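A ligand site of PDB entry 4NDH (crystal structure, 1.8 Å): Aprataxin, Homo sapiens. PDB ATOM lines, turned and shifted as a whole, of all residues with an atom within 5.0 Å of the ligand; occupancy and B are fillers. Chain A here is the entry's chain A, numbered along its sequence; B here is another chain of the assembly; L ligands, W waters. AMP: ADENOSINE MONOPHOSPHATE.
The backbone carbonyl oxygen (O) of Tyr 35 sits at hydrogen-bond distance from an oxygen (O2') of the ligand (3.4 Å). A ring nitrogen (NE2) of His 102 sits at hydrogen-bond distance from an oxygen (O2P) of the ligand. The side-chain amino group (NZ) of Lys 37 sits at hydrogen-bond distance from an oxygen (O2') of the ligand (3.2 Å). A ring nitrogen (NE2) of His 100 is in hydrogen-bond range of an oxygen (O2P) of the ligand, at 2.7 Å. N1 of the ligand lies within hydrogen-bond range of OG of Ser 14, 2.7 Å away. An oxygen (O3') of the ligand lies within hydrogen-bond range of the side-chain carboxylate of Asp 33 (2.5 Å). The backbone NH (N) of Met 96 is in hydrogen-bond range of an oxygen (O3P) of the ligand. N of Lys 34 is in hydrogen-bond range of N3 of the ligand (3.3 Å). An oxygen (O3P) of the ligand is in hydrogen-bond range of the backbone NH of Ser 95, at 2.9 Å. A ring nitrogen (ND1) of His 91 is in hydrogen-bond range of an oxygen (O1P) of the ligand, at 2.8 Å.
NE2 of His 41 lies within hydrogen-bond range of ND1 of His 102 (2.9 Å). The backbone NH (N) of Leu 43 sits at hydrogen-bond distance from the backbone carbonyl oxygen (O) of Ile 31 (2.9 Å). The side-chain amino group of Lys 37 sits at hydrogen-bond distance from the backbone carbonyl oxygen of Tyr 35, 2.7 Å away. NZ of Lys 37 is in salt-bridge range of OP1 of DT 2 of chain B. The backbone NH (N) of Asp 33 sits at hydrogen-bond distance from the backbone carbonyl oxygen (O) of His 41 (3.0 Å). OD1 of Asp 33 is in hydrogen-bond range of N of Tyr 35, 2.8 Å away. The side-chain hydroxyl (OG) of Ser 14 is in hydrogen-bond range of the side-chain sulfur (SD) of Met 20 (3.4 Å). A ring nitrogen (ND1) of His 41 is in hydrogen-bond range of the backbone NH (N) of Lys 37, at 3.0 Å.
Merely in contact with the ligand: Gly 10, Leu 11, His 41, Leu 43, Pro 94 and DG 1 of chain B. 16 residues have an atom within 4 Å of the ligand: Gly 10, Leu 11, Ser 14, Asp 33, Lys 34, Tyr 35, Lys 37, His 41, Leu 43, His 91, Pro 94, Ser 95, Met 96, His 100, His 102 and DG 1 of chain B. The nearest printed residue that does not touch the ligand is Ile 31 (4.1 Å).
Water W2 lies within hydrogen-bond range of an oxygen (O2P) of the ligand (2.8 Å), the backbone NH (N) of His 91 (2.9 Å) and a ring nitrogen (NE2) of His 100 (3.5 Å). Water W4 lies within hydrogen-bond range of the side-chain amino group (NZ) of Lys 37 and an oxygen (O3') of the ligand. Water W3 lies within hydrogen-bond range of a nitrogen (N6) of the ligand, the backbone carbonyl oxygen of Gly 10 and the side-chain hydroxyl of Ser 14.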
ATOM      1  N   GLY A  10     -11.428  15.452  14.340  1.00  0.00           N
ATOM      2  CA  GLY A  10     -10.019  15.830  14.394  1.00  0.00           C
ATOM      3  C   GLY A  10      -9.456  16.519  13.160  1.00  0.00           C
ATOM      4  O   GLY A  10      -8.565  17.356  13.262  1.00  0.00           O
ATOM      5  N   LEU A  11      -9.972  16.166  11.984  1.00  0.00           N
ATOM      6  CA  LEU A  11      -9.472  16.788  10.754  1.00  0.00           C
ATOM      7  C   LEU A  11      -9.831  18.262  10.695  1.00  0.00           C
ATOM      8  O   LEU A  11      -9.101  19.046  10.100  1.00  0.00           O
ATOM      9  CB  LEU A  11     -10.010  16.075   9.501  1.00  0.00           C
ATOM     10  CG  LEU A  11      -9.673  14.602   9.328  1.00  0.00           C
ATOM     11  CD1 LEU A  11     -10.123  14.126   7.960  1.00  0.00           C
ATOM     12  CD2 LEU A  11      -8.176  14.384   9.499  1.00  0.00           C
ATOM     13  N   SER A  14      -6.849  19.791  12.448  1.00  0.00           N
ATOM     14  CA  SER A  14      -5.595  19.682  11.700  1.00  0.00           C
ATOM     15  C   SER A  14      -5.550  20.506  10.402  1.00  0.00           C
ATOM     16  O   SER A  14      -4.499  21.039  10.033  1.00  0.00           O
ATOM     17  CB  SER A  14      -5.283  18.218  11.387  1.00  0.00           C
ATOM     18  OG  SER A  14      -5.110  17.484  12.574  1.00  0.00           O
ATOM     19  N   MET A  20       0.834  21.598   9.906  1.00  0.00           N
ATOM     20  CA  MET A  20       0.437  20.392   9.208  1.00  0.00           C
ATOM     21  C   MET A  20       0.099  20.651   7.745  1.00  0.00           C
ATOM     22  O   MET A  20       0.001  19.717   6.956  1.00  0.00           O
ATOM     23  CB  MET A  20      -0.772  19.746   9.906  1.00  0.00           C
ATOM     24  CG  MET A  20      -0.484  19.341  11.336  1.00  0.00           C
ATOM     25  SD  MET A  20      -1.905  18.507  12.073  1.00  0.00           S
ATOM     26  CE  MET A  20      -1.276  18.090  13.688  1.00  0.00           C
ATOM     27  N   ILE A  31      -2.922  18.578   3.927  1.00  0.00           N
ATOM     28  CA  ILE A  31      -2.156  18.364   5.152  1.00  0.00           C
ATOM     29  C   ILE A  31      -1.465  17.004   5.132  1.00  0.00           C
ATOM     30  O   ILE A  31      -1.836  16.107   4.381  1.00  0.00           O
ATOM     31  CB  ILE A  31      -3.046  18.454   6.415  1.00  0.00           C
ATOM     32  CG1 ILE A  31      -4.108  17.345   6.399  1.00  0.00           C
ATOM     33  CG2 ILE A  31      -3.705  19.825   6.504  1.00  0.00           C
ATOM     34  CD1 ILE A  31      -4.923  17.241   7.705  1.00  0.00           C
ATOM     35  N   LYS A  32      -0.422  16.884   5.948  1.00  0.00           N
ATOM     36  CA  LYS A  32       0.180  15.587   6.194  1.00  0.00           C
ATOM     37  C   LYS A  32      -0.796  14.786   7.033  1.00  0.00           C
ATOM     38  O   LYS A  32      -1.369  15.311   7.990  1.00  0.00           O
ATOM     39  CB  LYS A  32       1.495  15.752   6.968  1.00  0.00           C
ATOM     40  CG  LYS A  32       2.560  16.508   6.205  1.00  0.00           C
ATOM     41  CD  LYS A  32       3.878  16.570   6.961  1.00  0.00           C
ATOM     42  CE  LYS A  32       3.789  17.412   8.220  1.00  0.00           C
ATOM     43  NZ  LYS A  32       5.130  17.544   8.888  1.00  0.00           N
ATOM     44  N   ASP A  33      -1.008  13.521   6.667  1.00  0.00           N
ATOM     45  CA  ASP A  33      -1.796  12.636   7.520  1.00  0.00           C
ATOM     46  C   ASP A  33      -1.069  12.520   8.850  1.00  0.00           C
ATOM     47  O   ASP A  33       0.153  12.388   8.893  1.00  0.00           O
ATOM     48  CB  ASP A  33      -1.892  11.255   6.873  1.00  0.00           C
ATOM     49  CG  ASP A  33      -2.953  10.397   7.512  1.00  0.00           C
ATOM     50  OD1 ASP A  33      -2.752   9.964   8.669  1.00  0.00           O
ATOM     51  OD2 ASP A  33      -3.994  10.149   6.875  1.00  0.00           O
ATOM     52  N   LYS A  34      -1.823  12.574   9.952  1.00  0.00           N
ATOM     53  CA  LYS A  34      -1.206  12.546  11.276  1.00  0.00           C
ATOM     54  C   LYS A  34      -0.632  11.171  11.613  1.00  0.00           C
ATOM     55  O   LYS A  34       0.277  11.046  12.444  1.00  0.00           O
ATOM     56  CB  LYS A  34      -2.225  12.977  12.330  1.00  0.00           C
ATOM     57  CG  LYS A  34      -1.628  13.164  13.719  1.00  0.00           C
ATOM     58  CD  LYS A  34      -2.603  13.885  14.631  1.00  0.00           C
ATOM     59  CE  LYS A  34      -2.071  13.973  16.045  1.00  0.00           C
ATOM     60  NZ  LYS A  34      -3.040  14.634  16.956  1.00  0.00           N
ATOM     61  N   TYR A  35      -1.180  10.142  10.986  1.00  0.00           N
ATOM     62  CA  TYR A  35      -0.757   8.770  11.210  1.00  0.00           C
ATOM     63  C   TYR A  35      -0.523   8.113   9.863  1.00  0.00           C
ATOM     64  O   TYR A  35      -1.277   7.218   9.470  1.00  0.00           O
ATOM     65  CB  TYR A  35      -1.827   8.006  11.975  1.00  0.00           C
ATOM     66  CG  TYR A  35      -2.220   8.700  13.250  1.00  0.00           C
ATOM     67  CD1 TYR A  35      -1.484   8.527  14.409  1.00  0.00           C
ATOM     68  CD2 TYR A  35      -3.329   9.541  13.301  1.00  0.00           C
ATOM     69  CE1 TYR A  35      -1.841   9.173  15.594  1.00  0.00           C
ATOM     70  CE2 TYR A  35      -3.695  10.189  14.474  1.00  0.00           C
ATOM     71  CZ  TYR A  35      -2.937  10.002  15.606  1.00  0.00           C
ATOM     72  OH  TYR A  35      -3.293  10.632  16.785  1.00  0.00           O
ATOM     73  N   LYS A  37       0.262   6.116   6.602  1.00  0.00           N
ATOM     74  CA  LYS A  37       0.295   4.673   6.416  1.00  0.00           C
ATOM     75  C   LYS A  37       1.303   4.268   5.332  1.00  0.00           C
ATOM     76  O   LYS A  37       1.371   3.101   4.946  1.00  0.00           O
ATOM     77  CB  LYS A  37      -1.101   4.144   6.086  1.00  0.00           C
ATOM     78  CG  LYS A  37      -2.143   4.468   7.167  1.00  0.00           C
ATOM     79  CD  LYS A  37      -1.686   3.986   8.545  1.00  0.00           C
ATOM     80  CE  LYS A  37      -2.804   4.078   9.591  1.00  0.00           C
ATOM     81  NZ  LYS A  37      -3.356   5.468   9.713  1.00  0.00           N
ATOM     82  N   HIS A  41       2.011  10.391   2.737  1.00  0.00           N
ATOM     83  CA  HIS A  41       0.580  10.228   2.928  1.00  0.00           C
ATOM     84  C   HIS A  41      -0.010  11.586   3.284  1.00  0.00           C
ATOM     85  O   HIS A  41       0.225  12.100   4.381  1.00  0.00           O
ATOM     86  CB  HIS A  41       0.304   9.187   4.030  1.00  0.00           C
ATOM     87  CG  HIS A  41      -1.142   8.795   4.151  1.00  0.00           C
ATOM     88  ND1 HIS A  41      -1.578   7.854   5.055  1.00  0.00           N
ATOM     89  CD2 HIS A  41      -2.252   9.238   3.513  1.00  0.00           C
ATOM     90  CE1 HIS A  41      -2.888   7.716   4.959  1.00  0.00           C
ATOM     91  NE2 HIS A  41      -3.326   8.545   4.022  1.00  0.00           N
ATOM     92  N   LEU A  43      -3.580  14.292   2.987  1.00  0.00           N
ATOM     93  CA  LEU A  43      -5.021  14.399   2.822  1.00  0.00           C
ATOM     94  C   LEU A  43      -5.325  15.731   2.164  1.00  0.00           C
ATOM     95  O   LEU A  43      -4.788  16.780   2.563  1.00  0.00           O
ATOM     96  CB  LEU A  43      -5.702  14.339   4.182  1.00  0.00           C
ATOM     97  CG  LEU A  43      -5.404  13.110   5.037  1.00  0.00           C
ATOM     98  CD1 LEU A  43      -6.095  13.257   6.390  1.00  0.00           C
ATOM     99  CD2 LEU A  43      -5.887  11.841   4.342  1.00  0.00           C
ATOM    100  N   HIS A  91     -11.876   6.340   1.248  1.00  0.00           N
ATOM    101  CA  HIS A  91     -12.370   5.145   1.912  1.00  0.00           C
ATOM    102  C   HIS A  91     -13.886   5.079   1.733  1.00  0.00           C
ATOM    103  O   HIS A  91     -14.561   6.093   1.839  1.00  0.00           O
ATOM    104  CB  HIS A  91     -11.991   5.169   3.394  1.00  0.00           C
ATOM    105  CG  HIS A  91     -10.558   4.805   3.648  1.00  0.00           C
ATOM    106  ND1 HIS A  91      -9.902   5.106   4.817  1.00  0.00           N
ATOM    107  CD2 HIS A  91      -9.671   4.130   2.882  1.00  0.00           C
ATOM    108  CE1 HIS A  91      -8.659   4.663   4.754  1.00  0.00           C
ATOM    109  NE2 HIS A  91      -8.491   4.060   3.592  1.00  0.00           N
ATOM    110  N   ILE A  93     -16.196   3.881   3.527  1.00  0.00           N
ATOM    111  CA  ILE A  93     -16.852   4.293   4.758  1.00  0.00           C
ATOM    112  C   ILE A  93     -15.777   4.946   5.625  1.00  0.00           C
ATOM    113  O   ILE A  93     -14.970   4.263   6.248  1.00  0.00           O
ATOM    114  CB  ILE A  93     -17.439   3.089   5.523  1.00  0.00           C
ATOM    115  CG1 ILE A  93     -18.330   2.232   4.625  1.00  0.00           C
ATOM    116  CG2 ILE A  93     -18.241   3.572   6.733  1.00  0.00           C
ATOM    117  CD1 ILE A  93     -18.831   0.959   5.284  1.00  0.00           C
ATOM    118  N   PRO A  94     -15.764   6.275   5.679  1.00  0.00           N
ATOM    119  CA  PRO A  94     -14.683   6.931   6.419  1.00  0.00           C
ATOM    120  C   PRO A  94     -14.972   6.946   7.912  1.00  0.00           C
ATOM    121  O   PRO A  94     -16.102   6.711   8.330  1.00  0.00           O
ATOM    122  CB  PRO A  94     -14.705   8.350   5.861  1.00  0.00           C
ATOM    123  CG  PRO A  94     -16.149   8.573   5.529  1.00  0.00           C
ATOM    124  CD  PRO A  94     -16.714   7.237   5.092  1.00  0.00           C
ATOM    125  N   SER A  95     -13.936   7.204   8.715  1.00  0.00           N
ATOM    126  CA  SER A  95     -14.089   7.318  10.160  1.00  0.00           C
ATOM    127  C   SER A  95     -14.154   8.783  10.560  1.00  0.00           C
ATOM    128  O   SER A  95     -14.907   9.169  11.464  1.00  0.00           O
ATOM    129  CB  SER A  95     -12.913   6.647  10.875  1.00  0.00           C
ATOM    130  OG  SER A  95     -12.970   5.230  10.778  1.00  0.00           O
ATOM    131  N   MET A  96     -13.354   9.602   9.889  1.00  0.00           N
ATOM    132  CA  MET A  96     -13.221  10.996  10.244  1.00  0.00           C
ATOM    133  C   MET A  96     -14.175  11.848   9.420  1.00  0.00           C
ATOM    134  O   MET A  96     -14.325  11.653   8.212  1.00  0.00           O
ATOM    135  CB  MET A  96     -11.776  11.453  10.006  1.00  0.00           C
ATOM    136  CG  MET A  96     -10.728  10.597  10.735  1.00  0.00           C
ATOM    137  SD  MET A  96     -10.705  10.862  12.514  1.00  0.00           S
ATOM    138  CE  MET A  96     -10.135  12.564  12.563  1.00  0.00           C
ATOM    139  N   HIS A 100     -12.297  14.122   2.609  1.00  0.00           N
ATOM    140  CA  HIS A 100     -10.850  14.210   2.434  1.00  0.00           C
ATOM    141  C   HIS A 100     -10.399  13.152   1.440  1.00  0.00           C
ATOM    142  O   HIS A 100     -10.830  11.997   1.508  1.00  0.00           O
ATOM    143  CB  HIS A 100     -10.120  14.013   3.770  1.00  0.00           C
ATOM    144  CG  HIS A 100     -10.593  12.815   4.552  1.00  0.00           C
ATOM    145  ND1 HIS A 100     -11.751  12.831   5.297  1.00  0.00           N
ATOM    146  CD2 HIS A 100     -10.062  11.577   4.685  1.00  0.00           C
ATOM    147  CE1 HIS A 100     -11.911  11.650   5.873  1.00  0.00           C
ATOM    148  NE2 HIS A 100     -10.914  10.870   5.510  1.00  0.00           N
ATOM    149  N   HIS A 102      -7.391  10.877   0.093  1.00  0.00           N
ATOM    150  CA  HIS A 102      -6.098  10.282   0.430  1.00  0.00           C
ATOM    151  C   HIS A 102      -5.155  10.337  -0.757  1.00  0.00           C
ATOM    152  O   HIS A 102      -5.520   9.950  -1.872  1.00  0.00           O
ATOM    153  CB  HIS A 102      -6.266   8.818   0.839  1.00  0.00           C
ATOM    154  CG  HIS A 102      -6.913   8.628   2.179  1.00  0.00           C
ATOM    155  ND1 HIS A 102      -6.177   8.522   3.337  1.00  0.00           N
ATOM    156  CD2 HIS A 102      -8.218   8.517   2.539  1.00  0.00           C
ATOM    157  CE1 HIS A 102      -7.012   8.361   4.366  1.00  0.00           C
ATOM    158  NE2 HIS A 102      -8.247   8.364   3.902  1.00  0.00           N
ATOM    159  N   PHE A 122      -6.902   0.223   2.320  1.00  0.00           N
ATOM    160  CA  PHE A 122      -6.169   0.798   1.195  1.00  0.00           C
ATOM    161  C   PHE A 122      -5.959  -0.173   0.041  1.00  0.00           C
ATOM    162  O   PHE A 122      -5.510   0.222  -1.037  1.00  0.00           O
ATOM    163  CB  PHE A 122      -4.808   1.338   1.660  1.00  0.00           C
ATOM    164  CG  PHE A 122      -4.913   2.571   2.479  1.00  0.00           C
ATOM    165  CD1 PHE A 122      -5.124   3.805   1.873  1.00  0.00           C
ATOM    166  CD2 PHE A 122      -4.845   2.522   3.868  1.00  0.00           C
ATOM    167  CE1 PHE A 122      -5.232   4.962   2.623  1.00  0.00           C
ATOM    168  CE2 PHE A 122      -4.958   3.672   4.620  1.00  0.00           C
ATOM    169  CZ  PHE A 122      -5.155   4.888   3.999  1.00  0.00           C
ATOM    170  OP3  DG B   1      -7.860   2.724  11.196  1.00  0.00           O
ATOM    171  P    DG B   1      -9.387   3.101  10.951  1.00  0.00           P
ATOM    172  OP1  DG B   1      -9.603   3.030   9.491  1.00  0.00           O
ATOM    173  OP2  DG B   1     -10.229   2.296  11.862  1.00  0.00           O
ATOM    174  O5'  DG B   1      -9.567   4.619  11.421  1.00  0.00           O
ATOM    175  C5'  DG B   1      -8.924   5.674  10.705  1.00  0.00           C
ATOM    176  C4'  DG B   1      -8.531   6.754  11.679  1.00  0.00           C
ATOM    177  O4'  DG B   1      -9.725   7.278  12.294  1.00  0.00           O
ATOM    178  C3'  DG B   1      -7.714   6.251  12.853  1.00  0.00           C
ATOM    179  O3'  DG B   1      -6.346   6.252  12.519  1.00  0.00           O
ATOM    180  C2'  DG B   1      -8.017   7.250  13.948  1.00  0.00           C
ATOM    181  C1'  DG B   1      -9.496   7.444  13.679  1.00  0.00           C
ATOM    182  N9   DG B   1     -10.423   6.596  14.427  1.00  0.00           N
ATOM    183  C8   DG B   1     -11.317   5.685  13.928  1.00  0.00           C
ATOM    184  N7   DG B   1     -12.019   5.113  14.872  1.00  0.00           N
ATOM    185  C5   DG B   1     -11.553   5.655  16.048  1.00  0.00           C
ATOM    186  C6   DG B   1     -11.923   5.415  17.398  1.00  0.00           C
ATOM    187  O6   DG B   1     -12.802   4.651  17.820  1.00  0.00           O
ATOM    188  N1   DG B   1     -11.189   6.195  18.285  1.00  0.00           N
ATOM    189  C2   DG B   1     -10.213   7.089  17.921  1.00  0.00           C
ATOM    190  N2   DG B   1      -9.606   7.733  18.921  1.00  0.00           N
ATOM    191  N3   DG B   1      -9.851   7.330  16.666  1.00  0.00           N
ATOM    192  C4   DG B   1     -10.551   6.567  15.794  1.00  0.00           C
ATOM    193  P    DT B   2      -5.371   5.145  13.134  1.00  0.00           P
ATOM    194  OP1  DT B   2      -4.062   5.286  12.458  1.00  0.00           O
ATOM    195  OP2  DT B   2      -6.092   3.842  13.102  1.00  0.00           O
ATOM    196  O5'  DT B   2      -5.231   5.561  14.669  1.00  0.00           O
ATOM    197  C5'  DT B   2      -4.727   6.862  14.983  1.00  0.00           C
ATOM    198  C4'  DT B   2      -4.703   7.078  16.483  1.00  0.00           C
ATOM    199  O4'  DT B   2      -6.018   6.788  17.031  1.00  0.00           O
ATOM    200  C3'  DT B   2      -3.722   6.184  17.216  1.00  0.00           C
ATOM    201  O3'  DT B   2      -3.094   6.914  18.239  1.00  0.00           O
ATOM    202  C2'  DT B   2      -4.589   5.071  17.778  1.00  0.00           C
ATOM    203  C1'  DT B   2      -5.900   5.805  18.039  1.00  0.00           C
ATOM    204  N1   DT B   2      -7.085   4.916  17.942  1.00  0.00           N
ATOM    205  C2   DT B   2      -7.768   4.618  19.088  1.00  0.00           C
ATOM    206  O2   DT B   2      -7.451   5.037  20.183  1.00  0.00           O
ATOM    207  N3   DT B   2      -8.852   3.805  18.909  1.00  0.00           N
ATOM    208  C4   DT B   2      -9.298   3.269  17.720  1.00  0.00           C
ATOM    209  O4   DT B   2     -10.297   2.546  17.687  1.00  0.00           O
ATOM    210  C5   DT B   2      -8.538   3.626  16.541  1.00  0.00           C
ATOM    211  C7   DT B   2      -8.932   3.112  15.195  1.00  0.00           C
ATOM    212  C6   DT B   2      -7.474   4.427  16.714  1.00  0.00           C
HETATM  213  P   AMP L   1     -10.707   7.800   6.985  1.00  0.00           P
HETATM  214  O1P AMP L   1     -10.858   6.229   7.250  1.00  0.00           O
HETATM  215  O2P AMP L   1     -10.631   8.191   5.528  1.00  0.00           O
HETATM  216  O3P AMP L   1     -11.633   8.658   7.796  1.00  0.00           O
HETATM  217  O5' AMP L   1      -9.217   8.025   7.469  1.00  0.00           O
HETATM  218  C5' AMP L   1      -8.855   9.177   8.197  1.00  0.00           C
HETATM  219  C4' AMP L   1      -7.399   9.480   7.969  1.00  0.00           C
HETATM  220  O4' AMP L   1      -7.054  10.626   8.753  1.00  0.00           O
HETATM  221  C3' AMP L   1      -6.445   8.361   8.356  1.00  0.00           C
HETATM  222  O3' AMP L   1      -5.476   8.209   7.325  1.00  0.00           O
HETATM  223  C2' AMP L   1      -5.799   8.843   9.664  1.00  0.00           C
HETATM  224  O2' AMP L   1      -4.457   8.461   9.811  1.00  0.00           O
HETATM  225  C1' AMP L   1      -5.938  10.366   9.572  1.00  0.00           C
HETATM  226  N9  AMP L   1      -6.145  11.053  10.843  1.00  0.00           N
HETATM  227  C8  AMP L   1      -6.773  10.611  11.942  1.00  0.00           C
HETATM  228  N7  AMP L   1      -6.789  11.577  12.892  1.00  0.00           N
HETATM  229  C5  AMP L   1      -6.164  12.653  12.380  1.00  0.00           C
HETATM  230  C6  AMP L   1      -5.828  14.013  12.848  1.00  0.00           C
HETATM  231  N6  AMP L   1      -6.176  14.415  14.084  1.00  0.00           N
HETATM  232  N1  AMP L   1      -5.168  14.824  11.982  1.00  0.00           N
HETATM  233  C2  AMP L   1      -4.828  14.429  10.744  1.00  0.00           C
HETATM  234  N3  AMP L   1      -5.095  13.203  10.250  1.00  0.00           N
HETATM  235  C4  AMP L   1      -5.751  12.301  11.020  1.00  0.00           C
HETATM  236  O   HOH W   1      -8.585  12.904  16.124  1.00  0.00           O
HETATM  237  O   HOH W   2     -11.615   8.608   2.961  1.00  0.00           O
HETATM  238  O   HOH W   3      -6.574  17.018  15.447  1.00  0.00           O
HETATM  239  O   HOH W   4      -5.225   5.431   7.663  1.00  0.00           O
